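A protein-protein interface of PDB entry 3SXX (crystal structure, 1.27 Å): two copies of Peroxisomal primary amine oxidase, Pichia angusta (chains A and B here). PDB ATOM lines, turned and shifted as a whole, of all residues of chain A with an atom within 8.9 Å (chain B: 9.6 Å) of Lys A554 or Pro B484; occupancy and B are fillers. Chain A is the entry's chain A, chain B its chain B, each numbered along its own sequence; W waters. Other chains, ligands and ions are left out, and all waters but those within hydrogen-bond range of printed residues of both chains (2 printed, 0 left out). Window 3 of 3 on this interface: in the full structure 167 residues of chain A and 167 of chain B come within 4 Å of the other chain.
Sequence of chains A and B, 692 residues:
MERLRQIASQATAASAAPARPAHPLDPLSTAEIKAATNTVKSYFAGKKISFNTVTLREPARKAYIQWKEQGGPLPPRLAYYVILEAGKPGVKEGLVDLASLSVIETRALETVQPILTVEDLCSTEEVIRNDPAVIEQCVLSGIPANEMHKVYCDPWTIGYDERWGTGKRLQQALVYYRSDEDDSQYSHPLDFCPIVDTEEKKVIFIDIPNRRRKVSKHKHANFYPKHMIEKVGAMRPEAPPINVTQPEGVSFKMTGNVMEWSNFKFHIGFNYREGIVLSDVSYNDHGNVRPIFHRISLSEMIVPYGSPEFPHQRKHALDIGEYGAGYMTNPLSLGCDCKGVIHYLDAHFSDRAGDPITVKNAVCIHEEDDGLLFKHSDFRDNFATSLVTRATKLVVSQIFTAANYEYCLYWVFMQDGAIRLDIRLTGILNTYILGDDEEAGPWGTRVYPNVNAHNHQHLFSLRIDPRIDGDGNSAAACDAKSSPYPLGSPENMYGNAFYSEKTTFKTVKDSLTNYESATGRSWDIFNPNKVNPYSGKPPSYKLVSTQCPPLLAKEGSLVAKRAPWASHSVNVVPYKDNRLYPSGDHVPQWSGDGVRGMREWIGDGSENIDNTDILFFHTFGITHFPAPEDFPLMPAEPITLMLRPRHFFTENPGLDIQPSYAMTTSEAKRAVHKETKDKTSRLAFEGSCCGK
The side-chain hydroxyl (OG) of Ser B482 sits at hydrogen-bond distance from the backbone carbonyl oxygen (O) of Leu A552 (2.6 Å). NZ of Lys A554 lies within hydrogen-bond range of O of Ser B483. The backbone carbonyl oxygen (O) of Tyr B485 is in hydrogen-bond range of the side-chain amino group (NZ) of Lys A554. The backbone carbonyl oxygen (O) of Gly B495 lies within hydrogen-bond range of the backbone NH (N) of Lys A554 (2.9 Å).
OD1 of Asn B492 sits close to N of Gly B495 (3.4 Å). The backbone NH (N) of Ser B483 is in hydrogen-bond range of the backbone carbonyl oxygen (O) of Ala B497, 2.9 Å away. The backbone NH of Lys B481 sits at hydrogen-bond distance from the backbone carbonyl oxygen of Tyr B499 (2.9 Å). The backbone carbonyl oxygen (O) of Pro A304 is in hydrogen-bond range of the backbone NH (N) of Gln A457 (3.0 Å). N of Leu A552 is in hydrogen-bond range of OE1 of Gln A457 (3.1 Å). OG of Ser A557 sits at hydrogen-bond distance from O of Lys A554 (2.7 Å).
Among the printed residues, merely in contact across the chains: Ser A557 with Tyr B494 (3.2 Å), Trp A443 with Phe B498 (3.3 Å), Ala A553 with Gly B495 (3.3 Å), Leu A552 with Phe B498 (3.5 Å), Pro A442 with Tyr B499 (3.5 Å), Glu A555 with Leu B487 (3.6 Å), Gly A556 with Leu B487 (3.6 Å), Trp A443 with Ala B497 (3.7 Å), Lys A554 with Ser B482 (3.8 Å), Gln A457 with Phe B498 (3.9 Å), Pro A304 with Phe B498 (3.9 Å), Trp A443 with Ser B483 (3.9 Å) and Lys A554 with Pro B484 (3.9 Å).
Of the printed residues of chain B, Lys A554 touches Ser B482, Ser B483, Pro B484, Tyr B485 and Gly B495. Printed residues of chain A within 4 Å of Pro B484: Lys A554. Ala A553 touches one residue of chain B. Of the printed residues of chain A, Gly B495 touches Ala A553 (3.3 Å) and Lys A554 (2.9 Å). Printed residues of chain B within 4 Å of Gln A457: Phe B498 (3.9 Å). The nearest printed residue of chain A that does not touch Pro B484 is Trp A443 (5.7 Å). The nearest printed residue of chain A that does not touch Tyr B499 is Trp A443 (4.05 Å).
Hydrophobic or aromatic side chains of chain A within 4 Å of the printed part of chain B: Pro A442, Trp A443, Leu A552 and Ala A553. Of the 19 printed residues of chain B, 10 touch a printed residue of chain A. Among the printed residues, 17 pairs touch across the chains. Among the printed residues, no Asp or Glu carboxylate lies within 4 Å of a Lys or Arg side-chain nitrogen of the other chain.
No position is printed for both chains. Of the 17 pairs that touch across the chains among the printed residues, none has its exchanged pair printed and touching as well.
Water W1 lies within hydrogen-bond range of O of Tyr B494, N of Val A559 and N of Leu A558. Water W2 bridges OG of Ser B482 (2.9 Å) and O of Leu A552 (3.0 Å).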
ATOM      1  N   PRO A 304      30.937  29.852  -4.717  1.00  0.00           N
ATOM      2  CA  PRO A 304      30.453  28.712  -5.492  1.00  0.00           C
ATOM      3  C   PRO A 304      31.346  28.420  -6.709  1.00  0.00           C
ATOM      4  O   PRO A 304      31.587  29.291  -7.571  1.00  0.00           O
ATOM      5  CB  PRO A 304      29.062  29.186  -5.922  1.00  0.00           C
ATOM      6  CG  PRO A 304      29.203  30.681  -6.028  1.00  0.00           C
ATOM      7  CD  PRO A 304      30.079  31.037  -4.861  1.00  0.00           C
ATOM      8  N   PRO A 442      35.004  23.998 -20.473  1.00  0.00           N
ATOM      9  CA  PRO A 442      34.744  25.397 -20.226  1.00  0.00           C
ATOM     10  C   PRO A 442      34.666  25.736 -18.745  1.00  0.00           C
ATOM     11  O   PRO A 442      34.479  26.926 -18.392  1.00  0.00           O
ATOM     12  CB  PRO A 442      33.367  25.594 -20.876  1.00  0.00           C
ATOM     13  CG  PRO A 442      32.732  24.296 -20.721  1.00  0.00           C
ATOM     14  CD  PRO A 442      33.791  23.267 -20.882  1.00  0.00           C
ATOM     15  N   TRP A 443      34.845  24.749 -17.847  1.00  0.00           N
ATOM     16  CA  TRP A 443      34.570  24.971 -16.432  1.00  0.00           C
ATOM     17  C   TRP A 443      35.799  25.382 -15.613  1.00  0.00           C
ATOM     18  O   TRP A 443      35.676  25.636 -14.418  1.00  0.00           O
ATOM     19  CB  TRP A 443      33.964  23.732 -15.755  1.00  0.00           C
ATOM     20  CG  TRP A 443      32.915  23.052 -16.592  1.00  0.00           C
ATOM     21  CD1 TRP A 443      32.932  21.736 -16.975  1.00  0.00           C
ATOM     22  CD2 TRP A 443      31.729  23.643 -17.166  1.00  0.00           C
ATOM     23  NE1 TRP A 443      31.806  21.465 -17.737  1.00  0.00           N
ATOM     24  CE2 TRP A 443      31.049  22.607 -17.863  1.00  0.00           C
ATOM     25  CE3 TRP A 443      31.151  24.932 -17.121  1.00  0.00           C
ATOM     26  CZ2 TRP A 443      29.841  22.824 -18.551  1.00  0.00           C
ATOM     27  CZ3 TRP A 443      29.942  25.160 -17.822  1.00  0.00           C
ATOM     28  CH2 TRP A 443      29.332  24.114 -18.532  1.00  0.00           C
ATOM     29  N   GLN A 457      32.835  31.935  -8.139  1.00  0.00           N
ATOM     30  CA  GLN A 457      32.581  33.297  -7.674  1.00  0.00           C
ATOM     31  C   GLN A 457      33.008  33.425  -6.228  1.00  0.00           C
ATOM     32  O   GLN A 457      33.007  32.416  -5.513  1.00  0.00           O
ATOM     33  CB  GLN A 457      31.062  33.601  -7.805  1.00  0.00           C
ATOM     34  CG  GLN A 457      30.493  33.355  -9.209  1.00  0.00           C
ATOM     35  CD  GLN A 457      29.108  33.854  -9.369  1.00  0.00           C
ATOM     36  OE1 GLN A 457      28.157  33.154  -8.999  1.00  0.00           O
ATOM     37  NE2 GLN A 457      28.931  35.087  -9.833  1.00  0.00           N
ATOM     38  N   LEU A 551      24.196  35.851  -9.249  1.00  0.00           N
ATOM     39  CA  LEU A 551      24.507  34.493  -8.820  1.00  0.00           C
ATOM     40  C   LEU A 551      24.372  33.600 -10.025  1.00  0.00           C
ATOM     41  O   LEU A 551      23.294  33.536 -10.657  1.00  0.00           O
ATOM     42  CB  LEU A 551      23.556  34.083  -7.701  1.00  0.00           C
ATOM     43  CG  LEU A 551      23.806  32.667  -7.152  1.00  0.00           C
ATOM     44  CD1 LEU A 551      25.149  32.570  -6.460  1.00  0.00           C
ATOM     45  CD2 LEU A 551      22.631  32.274  -6.226  1.00  0.00           C
ATOM     46  N   LEU A 552      25.437  32.905 -10.426  1.00  0.00           N
ATOM     47  CA  LEU A 552      25.397  32.125 -11.686  1.00  0.00           C
ATOM     48  C   LEU A 552      24.726  30.778 -11.481  1.00  0.00           C
ATOM     49  O   LEU A 552      24.113  30.251 -12.424  1.00  0.00           O
ATOM     50  CB  LEU A 552      26.798  32.015 -12.279  1.00  0.00           C
ATOM     51  CG  LEU A 552      27.307  33.387 -12.773  1.00  0.00           C
ATOM     52  CD1 LEU A 552      28.805  33.334 -13.005  1.00  0.00           C
ATOM     53  CD2 LEU A 552      26.534  33.831 -14.029  1.00  0.00           C
ATOM     54  N   ALA A 553      24.799  30.187 -10.297  1.00  0.00           N
ATOM     55  CA  ALA A 553      24.095  28.919 -10.055  1.00  0.00           C
ATOM     56  C   ALA A 553      22.599  29.176 -10.195  1.00  0.00           C
ATOM     57  O   ALA A 553      22.075  30.229  -9.820  1.00  0.00           O
ATOM     58  CB  ALA A 553      24.427  28.452  -8.646  1.00  0.00           C
ATOM     59  N   LYS A 554      21.890  28.176 -10.731  1.00  0.00           N
ATOM     60  CA  LYS A 554      20.502  28.446 -11.087  1.00  0.00           C
ATOM     61  C   LYS A 554      19.547  28.366  -9.934  1.00  0.00           C
ATOM     62  O   LYS A 554      19.863  27.874  -8.863  1.00  0.00           O
ATOM     63  CB  LYS A 554      20.061  27.529 -12.190  1.00  0.00           C
ATOM     64  CG  LYS A 554      20.799  27.840 -13.458  1.00  0.00           C
ATOM     65  CD  LYS A 554      20.548  26.794 -14.538  1.00  0.00           C
ATOM     66  CE  LYS A 554      21.320  27.188 -15.798  1.00  0.00           C
ATOM     67  NZ  LYS A 554      20.544  26.823 -16.996  1.00  0.00           N
ATOM     68  N   GLU A 555      18.363  28.909 -10.131  1.00  0.00           N
ATOM     69  CA  GLU A 555      17.349  28.830  -9.077  1.00  0.00           C
ATOM     70  C   GLU A 555      17.083  27.374  -8.748  1.00  0.00           C
ATOM     71  O   GLU A 555      17.021  26.498  -9.630  1.00  0.00           O
ATOM     72  CB  GLU A 555      16.039  29.500  -9.515  1.00  0.00           C
ATOM     73  CG  GLU A 555      16.215  30.900 -10.101  1.00  0.00           C
ATOM     74  CD  GLU A 555      14.913  31.466 -10.612  1.00  0.00           C
ATOM     75  OE1 GLU A 555      14.068  31.805  -9.757  1.00  0.00           O
ATOM     76  OE2 GLU A 555      14.705  31.514 -11.856  1.00  0.00           O
ATOM     77  N   GLY A 556      16.960  27.092  -7.457  1.00  0.00           N
ATOM     78  CA  GLY A 556      16.725  25.746  -7.052  1.00  0.00           C
ATOM     79  C   GLY A 556      17.995  24.943  -6.899  1.00  0.00           C
ATOM     80  O   GLY A 556      17.972  23.807  -6.384  1.00  0.00           O
ATOM     81  N   SER A 557      19.155  25.519  -7.280  1.00  0.00           N
ATOM     82  CA  SER A 557      20.441  24.832  -7.016  1.00  0.00           C
ATOM     83  C   SER A 557      20.784  24.786  -5.517  1.00  0.00           C
ATOM     84  O   SER A 557      20.299  25.588  -4.743  1.00  0.00           O
ATOM     85  CB  SER A 557      21.590  25.545  -7.705  1.00  0.00           C
ATOM     86  OG  SER A 557      21.780  26.863  -7.248  1.00  0.00           O
ATOM     87  N   LEU A 558      21.693  23.878  -5.153  1.00  0.00           N
ATOM     88  CA  LEU A 558      22.102  23.802  -3.824  1.00  0.00           C
ATOM     89  C   LEU A 558      22.739  25.181  -3.374  1.00  0.00           C
ATOM     90  O   LEU A 558      22.499  25.660  -2.252  1.00  0.00           O
ATOM     91  CB  LEU A 558      23.016  22.625  -3.872  1.00  0.00           C
ATOM     92  CG  LEU A 558      23.710  22.391  -2.614  1.00  0.00           C
ATOM     93  CD1 LEU A 558      22.686  22.103  -1.507  1.00  0.00           C
ATOM     94  CD2 LEU A 558      24.710  21.206  -2.799  1.00  0.00           C
ATOM     95  N   VAL A 559      23.538  25.797  -4.264  1.00  0.00           N
ATOM     96  CA  VAL A 559      24.137  27.123  -3.970  1.00  0.00           C
ATOM     97  C   VAL A 559      23.025  28.149  -3.678  1.00  0.00           C
ATOM     98  O   VAL A 559      23.075  28.880  -2.676  1.00  0.00           O
ATOM     99  CB  VAL A 559      25.014  27.551  -5.149  1.00  0.00           C
ATOM    100  CG1 VAL A 559      25.395  28.997  -5.057  1.00  0.00           C
ATOM    101  CG2 VAL A 559      26.264  26.643  -5.198  1.00  0.00           C
ATOM    102  N   ALA A 560      22.036  28.255  -4.597  1.00  0.00           N
ATOM    103  CA  ALA A 560      21.027  29.293  -4.419  1.00  0.00           C
ATOM    104  C   ALA A 560      20.156  29.022  -3.185  1.00  0.00           C
ATOM    105  O   ALA A 560      19.661  29.966  -2.546  1.00  0.00           O
ATOM    106  CB  ALA A 560      20.169  29.383  -5.693  1.00  0.00           C
ATOM    107  N   LYS A 561      19.929  27.743  -2.885  1.00  0.00           N
ATOM    108  CA  LYS A 561      19.083  27.418  -1.713  1.00  0.00           C
ATOM    109  C   LYS A 561      19.794  27.686  -0.386  1.00  0.00           C
ATOM    110  O   LYS A 561      19.167  28.173   0.567  1.00  0.00           O
ATOM    111  CB  LYS A 561      18.661  25.955  -1.769  1.00  0.00           C
ATOM    112  CG  LYS A 561      17.700  25.657  -2.930  1.00  0.00           C
ATOM    113  CD  LYS A 561      17.495  24.157  -3.056  1.00  0.00           C
ATOM    114  CE  LYS A 561      16.767  23.594  -1.809  1.00  0.00           C
ATOM    115  NZ  LYS A 561      16.418  22.146  -2.092  1.00  0.00           N
ATOM    116  N   ARG A 562      21.105  27.397  -0.343  1.00  0.00           N
ATOM    117  CA  ARG A 562      21.877  27.602   0.917  1.00  0.00           C
ATOM    118  C   ARG A 562      22.255  29.051   1.113  1.00  0.00           C
ATOM    119  O   ARG A 562      22.580  29.429   2.246  1.00  0.00           O
ATOM    120  CB  ARG A 562      23.115  26.692   0.936  1.00  0.00           C
ATOM    121  CG  ARG A 562      22.706  25.215   1.084  1.00  0.00           C
ATOM    122  CD  ARG A 562      23.883  24.290   1.079  1.00  0.00           C
ATOM    123  NE  ARG A 562      24.524  24.423   2.423  1.00  0.00           N
ATOM    124  CZ  ARG A 562      25.830  24.402   2.713  1.00  0.00           C
ATOM    125  NH1 ARG A 562      26.751  24.297   1.753  1.00  0.00           N
ATOM    126  NH2 ARG A 562      26.275  24.522   4.012  1.00  0.00           N
ATOM    127  N   SER A 567      21.132  35.849  -4.262  1.00  0.00           N
ATOM    128  CA  SER A 567      20.535  36.019  -5.562  1.00  0.00           C
ATOM    129  C   SER A 567      20.007  37.429  -5.810  1.00  0.00           C
ATOM    130  O   SER A 567      19.562  37.673  -6.899  1.00  0.00           O
ATOM    131  CB  SER A 567      19.419  35.001  -5.713  1.00  0.00           C
ATOM    132  OG  SER A 567      18.572  35.109  -4.573  1.00  0.00           O
ATOM    133  N   LYS B 481      28.311  33.348 -17.980  1.00  0.00           N
ATOM    134  CA  LYS B 481      27.008  32.781 -18.260  1.00  0.00           C
ATOM    135  C   LYS B 481      26.853  31.462 -17.532  1.00  0.00           C
ATOM    136  O   LYS B 481      27.795  30.645 -17.500  1.00  0.00           O
ATOM    137  CB  LYS B 481      26.884  32.447 -19.762  1.00  0.00           C
ATOM    138  CG  LYS B 481      27.014  33.632 -20.682  1.00  0.00           C
ATOM    139  CD  LYS B 481      25.720  34.027 -21.161  1.00  0.00           C
ATOM    140  CE  LYS B 481      25.778  35.272 -21.969  1.00  0.00           C
ATOM    141  NZ  LYS B 481      24.439  35.889 -21.926  1.00  0.00           N
ATOM    142  N   SER B 482      25.681  31.218 -16.979  1.00  0.00           N
ATOM    143  CA  SER B 482      25.321  29.891 -16.527  1.00  0.00           C
ATOM    144  C   SER B 482      25.351  28.909 -17.693  1.00  0.00           C
ATOM    145  O   SER B 482      25.028  29.275 -18.819  1.00  0.00           O
ATOM    146  CB  SER B 482      23.903  29.951 -15.945  1.00  0.00           C
ATOM    147  OG  SER B 482      23.810  30.918 -14.921  1.00  0.00           O
ATOM    148  N   SER B 483      25.652  27.650 -17.433  1.00  0.00           N
ATOM    149  CA  SER B 483      25.457  26.629 -18.447  1.00  0.00           C
ATOM    150  C   SER B 483      24.026  26.699 -18.984  1.00  0.00           C
ATOM    151  O   SER B 483      23.090  26.918 -18.218  1.00  0.00           O
ATOM    152  CB  SER B 483      25.663  25.254 -17.802  1.00  0.00           C
ATOM    153  OG  SER B 483      25.253  24.249 -18.727  1.00  0.00           O
ATOM    154  N   PRO B 484      23.837  26.439 -20.283  1.00  0.00           N
ATOM    155  CA  PRO B 484      22.472  26.402 -20.811  1.00  0.00           C
ATOM    156  C   PRO B 484      21.700  25.152 -20.390  1.00  0.00           C
ATOM    157  O   PRO B 484      20.476  25.108 -20.537  1.00  0.00           O
ATOM    158  CB  PRO B 484      22.671  26.395 -22.320  1.00  0.00           C
ATOM    159  CG  PRO B 484      23.976  25.685 -22.513  1.00  0.00           C
ATOM    160  CD  PRO B 484      24.835  26.192 -21.323  1.00  0.00           C
ATOM    161  N   TYR B 485      22.371  24.136 -19.858  1.00  0.00           N
ATOM    162  CA  TYR B 485      21.672  22.936 -19.418  1.00  0.00           C
ATOM    163  C   TYR B 485      20.976  23.185 -18.091  1.00  0.00           C
ATOM    164  O   TYR B 485      21.521  23.844 -17.201  1.00  0.00           O
ATOM    165  CB  TYR B 485      22.638  21.742 -19.326  1.00  0.00           C
ATOM    166  CG  TYR B 485      23.112  21.286 -20.677  1.00  0.00           C
ATOM    167  CD1 TYR B 485      24.246  21.830 -21.263  1.00  0.00           C
ATOM    168  CD2 TYR B 485      22.366  20.335 -21.404  1.00  0.00           C
ATOM    169  CE1 TYR B 485      24.677  21.430 -22.531  1.00  0.00           C
ATOM    170  CE2 TYR B 485      22.751  19.945 -22.685  1.00  0.00           C
ATOM    171  CZ  TYR B 485      23.923  20.469 -23.204  1.00  0.00           C
ATOM    172  OH  TYR B 485      24.275  20.095 -24.477  1.00  0.00           O
ATOM    173  N   PRO B 486      19.779  22.645 -17.922  1.00  0.00           N
ATOM    174  CA  PRO B 486      19.014  22.929 -16.737  1.00  0.00           C
ATOM    175  C   PRO B 486      19.479  22.201 -15.495  1.00  0.00           C
ATOM    176  O   PRO B 486      20.124  21.144 -15.559  1.00  0.00           O
ATOM    177  CB  PRO B 486      17.583  22.488 -17.108  1.00  0.00           C
ATOM    178  CG  PRO B 486      17.790  21.399 -18.069  1.00  0.00           C
ATOM    179  CD  PRO B 486      19.029  21.828 -18.894  1.00  0.00           C
ATOM    180  N   LEU B 487      19.130  22.744 -14.350  1.00  0.00           N
ATOM    181  CA  LEU B 487      19.239  22.022 -13.089  1.00  0.00           C
ATOM    182  C   LEU B 487      18.646  20.617 -13.247  1.00  0.00           C
ATOM    183  O   LEU B 487      17.545  20.452 -13.828  1.00  0.00           O
ATOM    184  CB  LEU B 487      18.480  22.811 -12.047  1.00  0.00           C
ATOM    185  CG  LEU B 487      18.371  22.183 -10.664  1.00  0.00           C
ATOM    186  CD1 LEU B 487      19.703  22.151  -9.962  1.00  0.00           C
ATOM    187  CD2 LEU B 487      17.360  22.965  -9.813  1.00  0.00           C
ATOM    188  N   GLY B 488      19.349  19.592 -12.771  1.00  0.00           N
ATOM    189  CA  GLY B 488      18.838  18.238 -12.751  1.00  0.00           C
ATOM    190  C   GLY B 488      19.114  17.480 -14.066  1.00  0.00           C
ATOM    191  O   GLY B 488      18.797  16.292 -14.157  1.00  0.00           O
ATOM    192  N   SER B 489      19.756  18.113 -15.046  1.00  0.00           N
ATOM    193  CA  SER B 489      20.178  17.378 -16.241  1.00  0.00           C
ATOM    194  C   SER B 489      21.468  16.610 -15.943  1.00  0.00           C
ATOM    195  O   SER B 489      22.224  17.006 -15.043  1.00  0.00           O
ATOM    196  CB  SER B 489      20.361  18.355 -17.403  1.00  0.00           C
ATOM    197  OG  SER B 489      21.407  19.293 -17.114  1.00  0.00           O
ATOM    198  N   GLU B 491      24.095  16.985 -17.503  1.00  0.00           N
ATOM    199  CA  GLU B 491      25.149  17.915 -17.782  1.00  0.00           C
ATOM    200  C   GLU B 491      25.330  18.960 -16.687  1.00  0.00           C
ATOM    201  O   GLU B 491      26.394  19.635 -16.643  1.00  0.00           O
ATOM    202  CB  GLU B 491      24.846  18.671 -19.086  1.00  0.00           C
ATOM    203  CG  GLU B 491      24.843  17.789 -20.368  1.00  0.00           C
ATOM    204  CD  GLU B 491      23.530  17.097 -20.655  1.00  0.00           C
ATOM    205  OE1 GLU B 491      22.566  17.152 -19.878  1.00  0.00           O
ATOM    206  OE2 GLU B 491      23.406  16.528 -21.759  1.00  0.00           O
ATOM    207  N   ASN B 492      24.332  19.172 -15.820  1.00  0.00           N
ATOM    208  CA  ASN B 492      24.366  20.268 -14.832  1.00  0.00           C
ATOM    209  C   ASN B 492      23.500  19.827 -13.671  1.00  0.00           C
ATOM    210  O   ASN B 492      22.532  20.528 -13.298  1.00  0.00           O
ATOM    211  CB  ASN B 492      23.882  21.569 -15.489  1.00  0.00           C
ATOM    212  CG  ASN B 492      24.148  22.804 -14.667  1.00  0.00           C
ATOM    213  OD1 ASN B 492      24.999  22.780 -13.739  1.00  0.00           O
ATOM    214  ND2 ASN B 492      23.490  23.908 -15.021  1.00  0.00           N
ATOM    215  N   MET B 493      23.859  18.678 -13.067  1.00  0.00           N
ATOM    216  CA  MET B 493      22.936  18.032 -12.126  1.00  0.00           C
ATOM    217  C   MET B 493      22.524  18.972 -11.017  1.00  0.00           C
ATOM    218  O   MET B 493      21.350  19.061 -10.654  1.00  0.00           O
ATOM    219  CB  MET B 493      23.597  16.789 -11.556  1.00  0.00           C
ATOM    220  CG  MET B 493      22.714  16.042 -10.529  1.00  0.00           C
ATOM    221  SD  MET B 493      21.121  15.484 -11.226  1.00  0.00           S
ATOM    222  CE  MET B 493      21.691  14.445 -12.558  1.00  0.00           C
ATOM    223  N   TYR B 494      23.494  19.703 -10.446  1.00  0.00           N
ATOM    224  CA  TYR B 494      23.213  20.556  -9.282  1.00  0.00           C
ATOM    225  C   TYR B 494      23.081  22.026  -9.682  1.00  0.00           C
ATOM    226  O   TYR B 494      22.966  22.892  -8.822  1.00  0.00           O
ATOM    227  CB  TYR B 494      24.292  20.395  -8.185  1.00  0.00           C
ATOM    228  CG  TYR B 494      24.329  18.943  -7.695  1.00  0.00           C
ATOM    229  CD1 TYR B 494      25.134  18.003  -8.321  1.00  0.00           C
ATOM    230  CD2 TYR B 494      23.578  18.559  -6.557  1.00  0.00           C
ATOM    231  CE1 TYR B 494      25.229  16.682  -7.852  1.00  0.00           C
ATOM    232  CE2 TYR B 494      23.683  17.205  -6.080  1.00  0.00           C
ATOM    233  CZ  TYR B 494      24.494  16.324  -6.731  1.00  0.00           C
ATOM    234  OH  TYR B 494      24.651  15.024  -6.288  1.00  0.00           O
ATOM    235  N   GLY B 495      23.081  22.324 -10.990  1.00  0.00           N
ATOM    236  CA  GLY B 495      22.745  23.696 -11.442  1.00  0.00           C
ATOM    237  C   GLY B 495      23.819  24.726 -11.225  1.00  0.00           C
ATOM    238  O   GLY B 495      23.529  25.913 -11.336  1.00  0.00           O
ATOM    239  N   ASN B 496      25.059  24.310 -10.926  1.00  0.00           N
ATOM    240  CA  ASN B 496      26.124  25.256 -10.566  1.00  0.00           C
ATOM    241  C   ASN B 496      27.058  25.601 -11.738  1.00  0.00           C
ATOM    242  O   ASN B 496      27.921  26.489 -11.578  1.00  0.00           O
ATOM    243  CB  ASN B 496      26.950  24.668  -9.410  1.00  0.00           C
ATOM    244  CG  ASN B 496      27.637  23.402  -9.799  1.00  0.00           C
ATOM    245  OD1 ASN B 496      26.973  22.424 -10.192  1.00  0.00           O
ATOM    246  ND2 ASN B 496      28.958  23.360  -9.706  1.00  0.00           N
ATOM    247  N   ALA B 497      26.954  24.912 -12.869  1.00  0.00           N
ATOM    248  CA  ALA B 497      27.957  25.083 -13.933  1.00  0.00           C
ATOM    249  C   ALA B 497      27.902  26.522 -14.504  1.00  0.00           C
ATOM    250  O   ALA B 497      26.811  27.031 -14.797  1.00  0.00           O
ATOM    251  CB  ALA B 497      27.688  24.091 -15.065  1.00  0.00           C
ATOM    252  N   PHE B 498      29.054  27.112 -14.765  1.00  0.00           N
ATOM    253  CA  PHE B 498      29.082  28.379 -15.465  1.00  0.00           C
ATOM    254  C   PHE B 498      30.394  28.535 -16.179  1.00  0.00           C
ATOM    255  O   PHE B 498      31.416  27.907 -15.812  1.00  0.00           O
ATOM    256  CB  PHE B 498      28.749  29.564 -14.537  1.00  0.00           C
ATOM    257  CG  PHE B 498      29.829  29.948 -13.546  1.00  0.00           C
ATOM    258  CD1 PHE B 498      30.911  30.752 -13.967  1.00  0.00           C
ATOM    259  CD2 PHE B 498      29.787  29.502 -12.212  1.00  0.00           C
ATOM    260  CE1 PHE B 498      31.890  31.153 -13.063  1.00  0.00           C
ATOM    261  CE2 PHE B 498      30.716  29.956 -11.312  1.00  0.00           C
ATOM    262  CZ  PHE B 498      31.789  30.754 -11.735  1.00  0.00           C
ATOM    263  N   TYR B 499      30.423  29.412 -17.192  1.00  0.00           N
ATOM    264  CA  TYR B 499      31.554  29.574 -18.058  1.00  0.00           C
ATOM    265  C   TYR B 499      31.662  31.021 -18.523  1.00  0.00           C
ATOM    266  O   TYR B 499      30.780  31.847 -18.238  1.00  0.00           O
ATOM    267  CB  TYR B 499      31.484  28.617 -19.257  1.00  0.00           C
ATOM    268  CG  TYR B 499      30.369  28.934 -20.230  1.00  0.00           C
ATOM    269  CD1 TYR B 499      29.059  28.674 -19.944  1.00  0.00           C
ATOM    270  CD2 TYR B 499      30.653  29.534 -21.457  1.00  0.00           C
ATOM    271  CE1 TYR B 499      28.035  29.031 -20.809  1.00  0.00           C
ATOM    272  CE2 TYR B 499      29.629  29.890 -22.341  1.00  0.00           C
ATOM    273  CZ  TYR B 499      28.339  29.602 -22.044  1.00  0.00           C
ATOM    274  OH  TYR B 499      27.301  29.936 -22.888  1.00  0.00           O
ATOM    275  N   GLU B 501      31.683  33.224 -21.834  1.00  0.00           N
ATOM    276  CA  GLU B 501      31.407  33.228 -23.272  1.00  0.00           C
ATOM    277  C   GLU B 501      32.223  34.358 -23.892  1.00  0.00           C
ATOM    278  O   GLU B 501      32.029  35.544 -23.574  1.00  0.00           O
ATOM    279  CB  GLU B 501      29.934  33.517 -23.474  1.00  0.00           C
ATOM    280  CG  GLU B 501      29.559  33.604 -24.934  1.00  0.00           C
ATOM    281  CD  GLU B 501      28.105  33.673 -25.047  1.00  0.00           C
ATOM    282  OE1 GLU B 501      27.522  34.715 -24.694  1.00  0.00           O
ATOM    283  OE2 GLU B 501      27.544  32.628 -25.369  1.00  0.00           O
HETATM  284  O   HOH W   1      24.474  24.064  -6.689  1.00  0.00           O
HETATM  285  O   HOH W   2      21.369  31.145 -13.331  1.00  0.00           O
